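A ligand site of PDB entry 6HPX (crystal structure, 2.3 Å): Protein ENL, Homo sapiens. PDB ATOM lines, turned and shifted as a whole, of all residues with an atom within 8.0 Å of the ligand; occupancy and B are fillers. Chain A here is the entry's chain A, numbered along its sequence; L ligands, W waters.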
ATOM      1  N   GLU A  27      33.150 -10.081   5.587  1.00  0.00           N
ATOM      2  CA  GLU A  27      33.179  -8.586   5.628  1.00  0.00           C
ATOM      3  C   GLU A  27      31.941  -8.045   6.350  1.00  0.00           C
ATOM      4  O   GLU A  27      31.898  -6.822   6.567  1.00  0.00           O
ATOM      5  CB  GLU A  27      33.229  -7.973   4.240  1.00  0.00           C
ATOM      6  CG  GLU A  27      34.390  -8.466   3.416  1.00  0.00           C
ATOM      7  CD  GLU A  27      34.067  -9.673   2.558  1.00  0.00           C
ATOM      8  OE1 GLU A  27      34.918 -10.037   1.748  1.00  0.00           O
ATOM      9  OE2 GLU A  27      32.941 -10.228   2.709  1.00  0.00           O
ATOM     10  N   PHE A  29      28.826  -8.074   4.943  1.00  0.00           N
ATOM     11  CA  PHE A  29      27.794  -7.760   3.914  1.00  0.00           C
ATOM     12  C   PHE A  29      26.511  -8.543   4.246  1.00  0.00           C
ATOM     13  O   PHE A  29      26.571  -9.742   4.505  1.00  0.00           O
ATOM     14  CB  PHE A  29      28.290  -8.088   2.502  1.00  0.00           C
ATOM     15  CG  PHE A  29      29.517  -7.336   2.082  1.00  0.00           C
ATOM     16  CD1 PHE A  29      29.614  -5.972   2.279  1.00  0.00           C
ATOM     17  CD2 PHE A  29      30.563  -7.984   1.460  1.00  0.00           C
ATOM     18  CE1 PHE A  29      30.747  -5.278   1.877  1.00  0.00           C
ATOM     19  CE2 PHE A  29      31.708  -7.289   1.064  1.00  0.00           C
ATOM     20  CZ  PHE A  29      31.790  -5.926   1.276  1.00  0.00           C
ATOM     21  N   THR A  30      25.389  -7.841   4.297  1.00  0.00           N
ATOM     22  CA  THR A  30      24.088  -8.398   4.731  1.00  0.00           C
ATOM     23  C   THR A  30      23.242  -8.777   3.511  1.00  0.00           C
ATOM     24  O   THR A  30      22.314  -9.560   3.703  1.00  0.00           O
ATOM     25  CB  THR A  30      23.362  -7.397   5.637  1.00  0.00           C
ATOM     26  OG1 THR A  30      23.300  -6.153   4.939  1.00  0.00           O
ATOM     27  CG2 THR A  30      24.057  -7.203   6.964  1.00  0.00           C
ATOM     28  N   HIS A  31      23.549  -8.243   2.325  1.00  0.00           N
ATOM     29  CA  HIS A  31      22.690  -8.352   1.102  1.00  0.00           C
ATOM     30  C   HIS A  31      23.518  -8.693  -0.119  1.00  0.00           C
ATOM     31  O   HIS A  31      24.573  -8.010  -0.330  1.00  0.00           O
ATOM     32  CB  HIS A  31      21.941  -7.061   0.846  1.00  0.00           C
ATOM     33  CG  HIS A  31      20.881  -6.768   1.846  1.00  0.00           C
ATOM     34  ND1 HIS A  31      21.171  -6.330   3.112  1.00  0.00           N
ATOM     35  CD2 HIS A  31      19.528  -6.779   1.738  1.00  0.00           C
ATOM     36  CE1 HIS A  31      20.060  -6.149   3.780  1.00  0.00           C
ATOM     37  NE2 HIS A  31      19.028  -6.414   2.943  1.00  0.00           N
ATOM     38  N   TRP A  33      22.916  -8.174  -4.207  1.00  0.00           N
ATOM     39  CA  TRP A  33      22.129  -7.530  -5.275  1.00  0.00           C
ATOM     40  C   TRP A  33      22.774  -7.739  -6.648  1.00  0.00           C
ATOM     41  O   TRP A  33      23.979  -8.083  -6.740  1.00  0.00           O
ATOM     42  CB  TRP A  33      21.908  -6.041  -4.989  1.00  0.00           C
ATOM     43  CG  TRP A  33      23.140  -5.242  -4.730  1.00  0.00           C
ATOM     44  CD1 TRP A  33      23.585  -4.831  -3.512  1.00  0.00           C
ATOM     45  CD2 TRP A  33      23.951  -4.560  -5.703  1.00  0.00           C
ATOM     46  NE1 TRP A  33      24.674  -4.028  -3.648  1.00  0.00           N
ATOM     47  CE2 TRP A  33      24.945  -3.843  -4.974  1.00  0.00           C
ATOM     48  CE3 TRP A  33      23.970  -4.501  -7.099  1.00  0.00           C
ATOM     49  CZ2 TRP A  33      25.927  -3.081  -5.611  1.00  0.00           C
ATOM     50  CZ3 TRP A  33      24.955  -3.759  -7.728  1.00  0.00           C
ATOM     51  CH2 TRP A  33      25.912  -3.045  -6.987  1.00  0.00           C
ATOM     52  N   LEU A  56      28.590   2.555  -8.931  1.00  0.00           N
ATOM     53  CA  LEU A  56      28.282   2.055  -7.567  1.00  0.00           C
ATOM     54  C   LEU A  56      28.618   3.167  -6.557  1.00  0.00           C
ATOM     55  O   LEU A  56      29.416   4.027  -6.875  1.00  0.00           O
ATOM     56  CB  LEU A  56      29.093   0.779  -7.309  1.00  0.00           C
ATOM     57  CG  LEU A  56      28.547  -0.502  -7.921  1.00  0.00           C
ATOM     58  CD1 LEU A  56      28.318  -0.356  -9.419  1.00  0.00           C
ATOM     59  CD2 LEU A  56      29.497  -1.638  -7.652  1.00  0.00           C
ATOM     60  N   HIS A  57      28.017   3.125  -5.379  1.00  0.00           N
ATOM     61  CA  HIS A  57      28.416   3.935  -4.205  1.00  0.00           C
ATOM     62  C   HIS A  57      29.941   3.886  -4.036  1.00  0.00           C
ATOM     63  O   HIS A  57      30.530   2.792  -4.283  1.00  0.00           O
ATOM     64  CB  HIS A  57      27.702   3.412  -2.977  1.00  0.00           C
ATOM     65  CG  HIS A  57      27.856   4.285  -1.799  1.00  0.00           C
ATOM     66  ND1 HIS A  57      29.022   4.364  -1.121  1.00  0.00           N
ATOM     67  CD2 HIS A  57      26.981   5.106  -1.185  1.00  0.00           C
ATOM     68  CE1 HIS A  57      28.884   5.212  -0.116  1.00  0.00           C
ATOM     69  NE2 HIS A  57      27.638   5.677  -0.124  1.00  0.00           N
ATOM     70  N   ASP A  58      30.590   5.013  -3.708  1.00  0.00           N
ATOM     71  CA  ASP A  58      32.070   5.172  -3.868  1.00  0.00           C
ATOM     72  C   ASP A  58      32.786   4.362  -2.770  1.00  0.00           C
ATOM     73  O   ASP A  58      33.984   4.110  -2.932  1.00  0.00           O
ATOM     74  CB  ASP A  58      32.508   6.630  -3.942  1.00  0.00           C
ATOM     75  CG  ASP A  58      32.035   7.500  -2.792  1.00  0.00           C
ATOM     76  OD1 ASP A  58      32.014   7.008  -1.651  1.00  0.00           O
ATOM     77  OD2 ASP A  58      31.738   8.681  -3.041  1.00  0.00           O
ATOM     78  N   SER A  59      32.038   3.865  -1.782  1.00  0.00           N
ATOM     79  CA  SER A  59      32.497   2.860  -0.785  1.00  0.00           C
ATOM     80  C   SER A  59      32.941   1.561  -1.493  1.00  0.00           C
ATOM     81  O   SER A  59      33.816   0.861  -0.944  1.00  0.00           O
ATOM     82  CB  SER A  59      31.419   2.579   0.243  1.00  0.00           C
ATOM     83  OG  SER A  59      30.399   1.753  -0.291  1.00  0.00           O
ATOM     84  N   PHE A  60      32.386   1.261  -2.665  1.00  0.00           N
ATOM     85  CA  PHE A  60      32.780   0.073  -3.471  1.00  0.00           C
ATOM     86  C   PHE A  60      34.139   0.320  -4.105  1.00  0.00           C
ATOM     87  O   PHE A  60      34.415   1.419  -4.595  1.00  0.00           O
ATOM     88  CB  PHE A  60      31.733  -0.255  -4.545  1.00  0.00           C
ATOM     89  CG  PHE A  60      30.544  -0.997  -4.032  1.00  0.00           C
ATOM     90  CD1 PHE A  60      30.593  -2.374  -3.856  1.00  0.00           C
ATOM     91  CD2 PHE A  60      29.397  -0.329  -3.629  1.00  0.00           C
ATOM     92  CE1 PHE A  60      29.489  -3.060  -3.358  1.00  0.00           C
ATOM     93  CE2 PHE A  60      28.318  -1.013  -3.118  1.00  0.00           C
ATOM     94  CZ  PHE A  60      28.361  -2.379  -2.992  1.00  0.00           C
ATOM     95  N   PRO A  61      35.023  -0.711  -4.129  1.00  0.00           N
ATOM     96  CA  PRO A  61      36.256  -0.648  -4.915  1.00  0.00           C
ATOM     97  C   PRO A  61      35.965  -0.567  -6.425  1.00  0.00           C
ATOM     98  O   PRO A  61      34.988  -1.142  -6.854  1.00  0.00           O
ATOM     99  CB  PRO A  61      37.030  -1.941  -4.541  1.00  0.00           C
ATOM    100  CG  PRO A  61      35.990  -2.879  -3.868  1.00  0.00           C
ATOM    101  CD  PRO A  61      34.854  -1.981  -3.402  1.00  0.00           C
ATOM    102  N   ARG A  65      31.857   0.722 -12.888  1.00  0.00           N
ATOM    103  CA  ARG A  65      31.845  -0.612 -13.519  1.00  0.00           C
ATOM    104  C   ARG A  65      31.349  -0.476 -14.965  1.00  0.00           C
ATOM    105  O   ARG A  65      30.235   0.025 -15.182  1.00  0.00           O
ATOM    106  CB  ARG A  65      30.977  -1.573 -12.699  1.00  0.00           C
ATOM    107  CG  ARG A  65      31.392  -1.684 -11.238  1.00  0.00           C
ATOM    108  CD  ARG A  65      32.774  -2.307 -11.033  1.00  0.00           C
ATOM    109  NE  ARG A  65      33.113  -2.361  -9.631  1.00  0.00           N
ATOM    110  CZ  ARG A  65      32.687  -3.303  -8.769  1.00  0.00           C
ATOM    111  NH1 ARG A  65      33.027  -3.232  -7.502  1.00  0.00           N
ATOM    112  NH2 ARG A  65      31.917  -4.306  -9.184  1.00  0.00           N
ATOM    113  N   GLU A  76      26.858  -7.780  -6.784  1.00  0.00           N
ATOM    114  CA  GLU A  76      27.638  -7.345  -5.595  1.00  0.00           C
ATOM    115  C   GLU A  76      26.939  -7.838  -4.340  1.00  0.00           C
ATOM    116  O   GLU A  76      25.761  -8.159  -4.401  1.00  0.00           O
ATOM    117  CB  GLU A  76      27.774  -5.832  -5.576  1.00  0.00           C
ATOM    118  CG  GLU A  76      28.912  -5.293  -6.410  1.00  0.00           C
ATOM    119  CD  GLU A  76      30.282  -5.802  -6.011  1.00  0.00           C
ATOM    120  OE1 GLU A  76      30.397  -6.364  -4.892  1.00  0.00           O
ATOM    121  OE2 GLU A  76      31.244  -5.667  -6.839  1.00  0.00           O
ATOM    122  N   SER A  77      27.667  -7.895  -3.247  1.00  0.00           N
ATOM    123  CA  SER A  77      27.100  -7.891  -1.879  1.00  0.00           C
ATOM    124  C   SER A  77      27.390  -6.538  -1.261  1.00  0.00           C
ATOM    125  O   SER A  77      28.354  -5.874  -1.706  1.00  0.00           O
ATOM    126  CB  SER A  77      27.658  -9.024  -1.040  1.00  0.00           C
ATOM    127  OG  SER A  77      27.333 -10.272  -1.605  1.00  0.00           O
ATOM    128  N   GLY A  78      26.619  -6.144  -0.286  1.00  0.00           N
ATOM    129  CA  GLY A  78      26.795  -4.861   0.387  1.00  0.00           C
ATOM    130  C   GLY A  78      25.909  -4.722   1.571  1.00  0.00           C
ATOM    131  O   GLY A  78      25.314  -5.761   1.992  1.00  0.00           O
ATOM    132  N   TYR A  79      25.818  -3.503   2.107  1.00  0.00           N
ATOM    133  CA  TYR A  79      25.220  -3.179   3.425  1.00  0.00           C
ATOM    134  C   TYR A  79      23.896  -2.471   3.192  1.00  0.00           C
ATOM    135  O   TYR A  79      22.988  -2.652   3.981  1.00  0.00           O
ATOM    136  CB  TYR A  79      26.177  -2.329   4.271  1.00  0.00           C
ATOM    137  CG  TYR A  79      27.506  -2.970   4.608  1.00  0.00           C
ATOM    138  CD1 TYR A  79      27.599  -4.018   5.528  1.00  0.00           C
ATOM    139  CD2 TYR A  79      28.692  -2.486   4.051  1.00  0.00           C
ATOM    140  CE1 TYR A  79      28.833  -4.594   5.843  1.00  0.00           C
ATOM    141  CE2 TYR A  79      29.925  -3.053   4.366  1.00  0.00           C
ATOM    142  CZ  TYR A  79      29.998  -4.121   5.250  1.00  0.00           C
ATOM    143  OH  TYR A  79      31.241  -4.657   5.573  1.00  0.00           O
ATOM    144  N   ALA A  80      23.793  -1.650   2.146  1.00  0.00           N
ATOM    145  CA  ALA A  80      22.657  -0.739   1.931  1.00  0.00           C
ATOM    146  C   ALA A  80      22.440  -0.482   0.432  1.00  0.00           C
ATOM    147  O   ALA A  80      23.379  -0.661  -0.351  1.00  0.00           O
ATOM    148  CB  ALA A  80      22.877   0.545   2.675  1.00  0.00           C
ATOM    149  N   GLY A  81      21.237  -0.023   0.086  1.00  0.00           N
ATOM    150  CA  GLY A  81      20.926   0.552  -1.224  1.00  0.00           C
ATOM    151  C   GLY A  81      21.444   1.967  -1.355  1.00  0.00           C
ATOM    152  O   GLY A  81      21.886   2.545  -0.343  1.00  0.00           O
ATOM    153  N   PHE A  82      21.354   2.513  -2.565  1.00  0.00           N
ATOM    154  CA  PHE A  82      21.852   3.855  -2.952  1.00  0.00           C
ATOM    155  C   PHE A  82      21.298   4.165  -4.337  1.00  0.00           C
ATOM    156  O   PHE A  82      20.705   3.253  -4.972  1.00  0.00           O
ATOM    157  CB  PHE A  82      23.379   3.861  -2.930  1.00  0.00           C
ATOM    158  CG  PHE A  82      24.008   2.791  -3.795  1.00  0.00           C
ATOM    159  CD1 PHE A  82      24.220   1.505  -3.302  1.00  0.00           C
ATOM    160  CD2 PHE A  82      24.405   3.064  -5.096  1.00  0.00           C
ATOM    161  CE1 PHE A  82      24.743   0.516  -4.113  1.00  0.00           C
ATOM    162  CE2 PHE A  82      24.951   2.077  -5.904  1.00  0.00           C
ATOM    163  CZ  PHE A  82      25.121   0.798  -5.408  1.00  0.00           C
ATOM    164  N   ILE A  83      21.475   5.397  -4.804  1.00  0.00           N
ATOM    165  CA  ILE A  83      21.087   5.788  -6.176  1.00  0.00           C
ATOM    166  C   ILE A  83      22.296   5.552  -7.084  1.00  0.00           C
ATOM    167  O   ILE A  83      23.387   6.029  -6.754  1.00  0.00           O
ATOM    168  CB  ILE A  83      20.595   7.240  -6.237  1.00  0.00           C
ATOM    169  CG1 ILE A  83      19.454   7.507  -5.234  1.00  0.00           C
ATOM    170  CG2 ILE A  83      20.194   7.602  -7.657  1.00  0.00           C
ATOM    171  CD1 ILE A  83      18.174   6.715  -5.510  1.00  0.00           C
ATOM    172  N   LEU A 105      18.578   1.845  -6.565  1.00  0.00           N
ATOM    173  CA  LEU A 105      18.971   0.493  -6.117  1.00  0.00           C
ATOM    174  C   LEU A 105      18.617   0.307  -4.650  1.00  0.00           C
ATOM    175  O   LEU A 105      19.491   0.341  -3.841  1.00  0.00           O
ATOM    176  CB  LEU A 105      20.457   0.274  -6.356  1.00  0.00           C
ATOM    177  CG  LEU A 105      20.888  -1.178  -6.152  1.00  0.00           C
ATOM    178  CD1 LEU A 105      20.863  -1.937  -7.461  1.00  0.00           C
ATOM    179  CD2 LEU A 105      22.250  -1.245  -5.525  1.00  0.00           C
ATOM    180  N   LEU A 107      17.237  -2.039  -1.347  1.00  0.00           N
ATOM    181  CA  LEU A 107      17.296  -3.399  -0.755  1.00  0.00           C
ATOM    182  C   LEU A 107      16.025  -3.635   0.030  1.00  0.00           C
ATOM    183  O   LEU A 107      15.337  -2.679   0.296  1.00  0.00           O
ATOM    184  CB  LEU A 107      18.528  -3.524   0.151  1.00  0.00           C
ATOM    185  CG  LEU A 107      19.886  -3.128  -0.449  1.00  0.00           C
ATOM    186  CD1 LEU A 107      21.021  -3.552   0.473  1.00  0.00           C
ATOM    187  CD2 LEU A 107      20.092  -3.729  -1.817  1.00  0.00           C
HETATM  188  C1  LIG L   1      27.305   2.783   2.002  1.00  0.00           C
HETATM  189  N1  LIG L   1      27.784   3.822   2.810  1.00  0.00           N
HETATM  190  O1  LIG L   1      27.027  -1.643   0.619  1.00  0.00           O
HETATM  191  C2  LIG L   1      26.049   3.103   1.513  1.00  0.00           C
HETATM  192  C3  LIG L   1      26.822   4.718   2.782  1.00  0.00           C
HETATM  193  C4  LIG L   1      24.588   5.181   1.706  1.00  0.00           C
HETATM  194  C5  LIG L   1      27.754  -0.655   0.512  1.00  0.00           C
HETATM  195  N2  LIG L   1      29.041  -0.754   0.168  1.00  0.00           N
HETATM  196  C6  LIG L   1      29.770  -2.010   0.231  1.00  0.00           C
HETATM  197  C7  LIG L   1      31.200  -1.855   0.693  1.00  0.00           C
HETATM  198  C8  LIG L   1      32.215  -2.628   0.141  1.00  0.00           C
HETATM  199  C9  LIG L   1      33.526  -2.492   0.588  1.00  0.00           C
HETATM  200  C10 LIG L   1      33.842  -1.591   1.580  1.00  0.00           C
HETATM  201  C11 LIG L   1      32.818  -0.829   2.135  1.00  0.00           C
HETATM  202 CL1  LIG L   1      33.177   0.285   3.430  1.00  0.00          CL
HETATM  203  C12 LIG L   1      31.509  -0.955   1.698  1.00  0.00           C
HETATM  204  C13 LIG L   1      27.225   0.712   0.787  1.00  0.00           C
HETATM  205  C14 LIG L   1      27.911   1.584   1.644  1.00  0.00           C
HETATM  206  C15 LIG L   1      25.970   1.073   0.277  1.00  0.00           C
HETATM  207  C16 LIG L   1      25.359   2.262   0.648  1.00  0.00           C
HETATM  208  N3  LIG L   1      25.756   4.359   2.017  1.00  0.00           N
HETATM  209  C17 LIG L   1      23.556   5.121   2.807  1.00  0.00           C
HETATM  210  N4  LIG L   1      22.424   6.003   2.560  1.00  0.00           N
HETATM  211  C18 LIG L   1      21.389   5.409   1.698  1.00  0.00           C
HETATM  212  C19 LIG L   1      20.211   6.355   1.832  1.00  0.00           C
HETATM  213  C20 LIG L   1      20.397   7.003   3.227  1.00  0.00           C
HETATM  214  C21 LIG L   1      21.699   6.413   3.761  1.00  0.00           C
HETATM  215  O   HOH W   1      25.057  -2.335  -1.338  1.00  0.00           O
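OG of Ser 59 lies within hydrogen-bond range of N2 of the ligand.
O1 of the ligand lies within hydrogen-bond range of N of Tyr 79.
NE2 of His 57 sits close to N1 of the ligand, 3.5 Å away.
The side-chain hydroxyl (OH) of Tyr 79 is in hydrogen-bond range of the backbone carbonyl oxygen (O) of Glu 27, at 2.5 Å.
The backbone carbonyl oxygen (O) of Gly 78 sits at hydrogen-bond distance from the backbone NH (N) of Thr 30.
The backbone NH (N) of Gly 78 sits at hydrogen-bond distance from the backbone carbonyl oxygen (O) of His 31 (2.8 Å).
OG of Ser 59 sits at hydrogen-bond distance from ND1 of His 57 (3.1 Å).
Residues that only touch the ligand: Ala 80, Gly 78, Phe 60, Phe 29 and Gly 81.
Eight residues have an atom within 4 Å of the ligand: Phe 29, His 57, Ser 59, Phe 60, Gly 78, Tyr 79, Ala 80 and Gly 81.
Water W1 lies within hydrogen-bond range of the backbone carbonyl oxygen of Ala 80 (2.6 Å), an oxygen (O1) of the ligand (2.9 Å) and the indole nitrogen of Trp 33 (2.9 Å).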
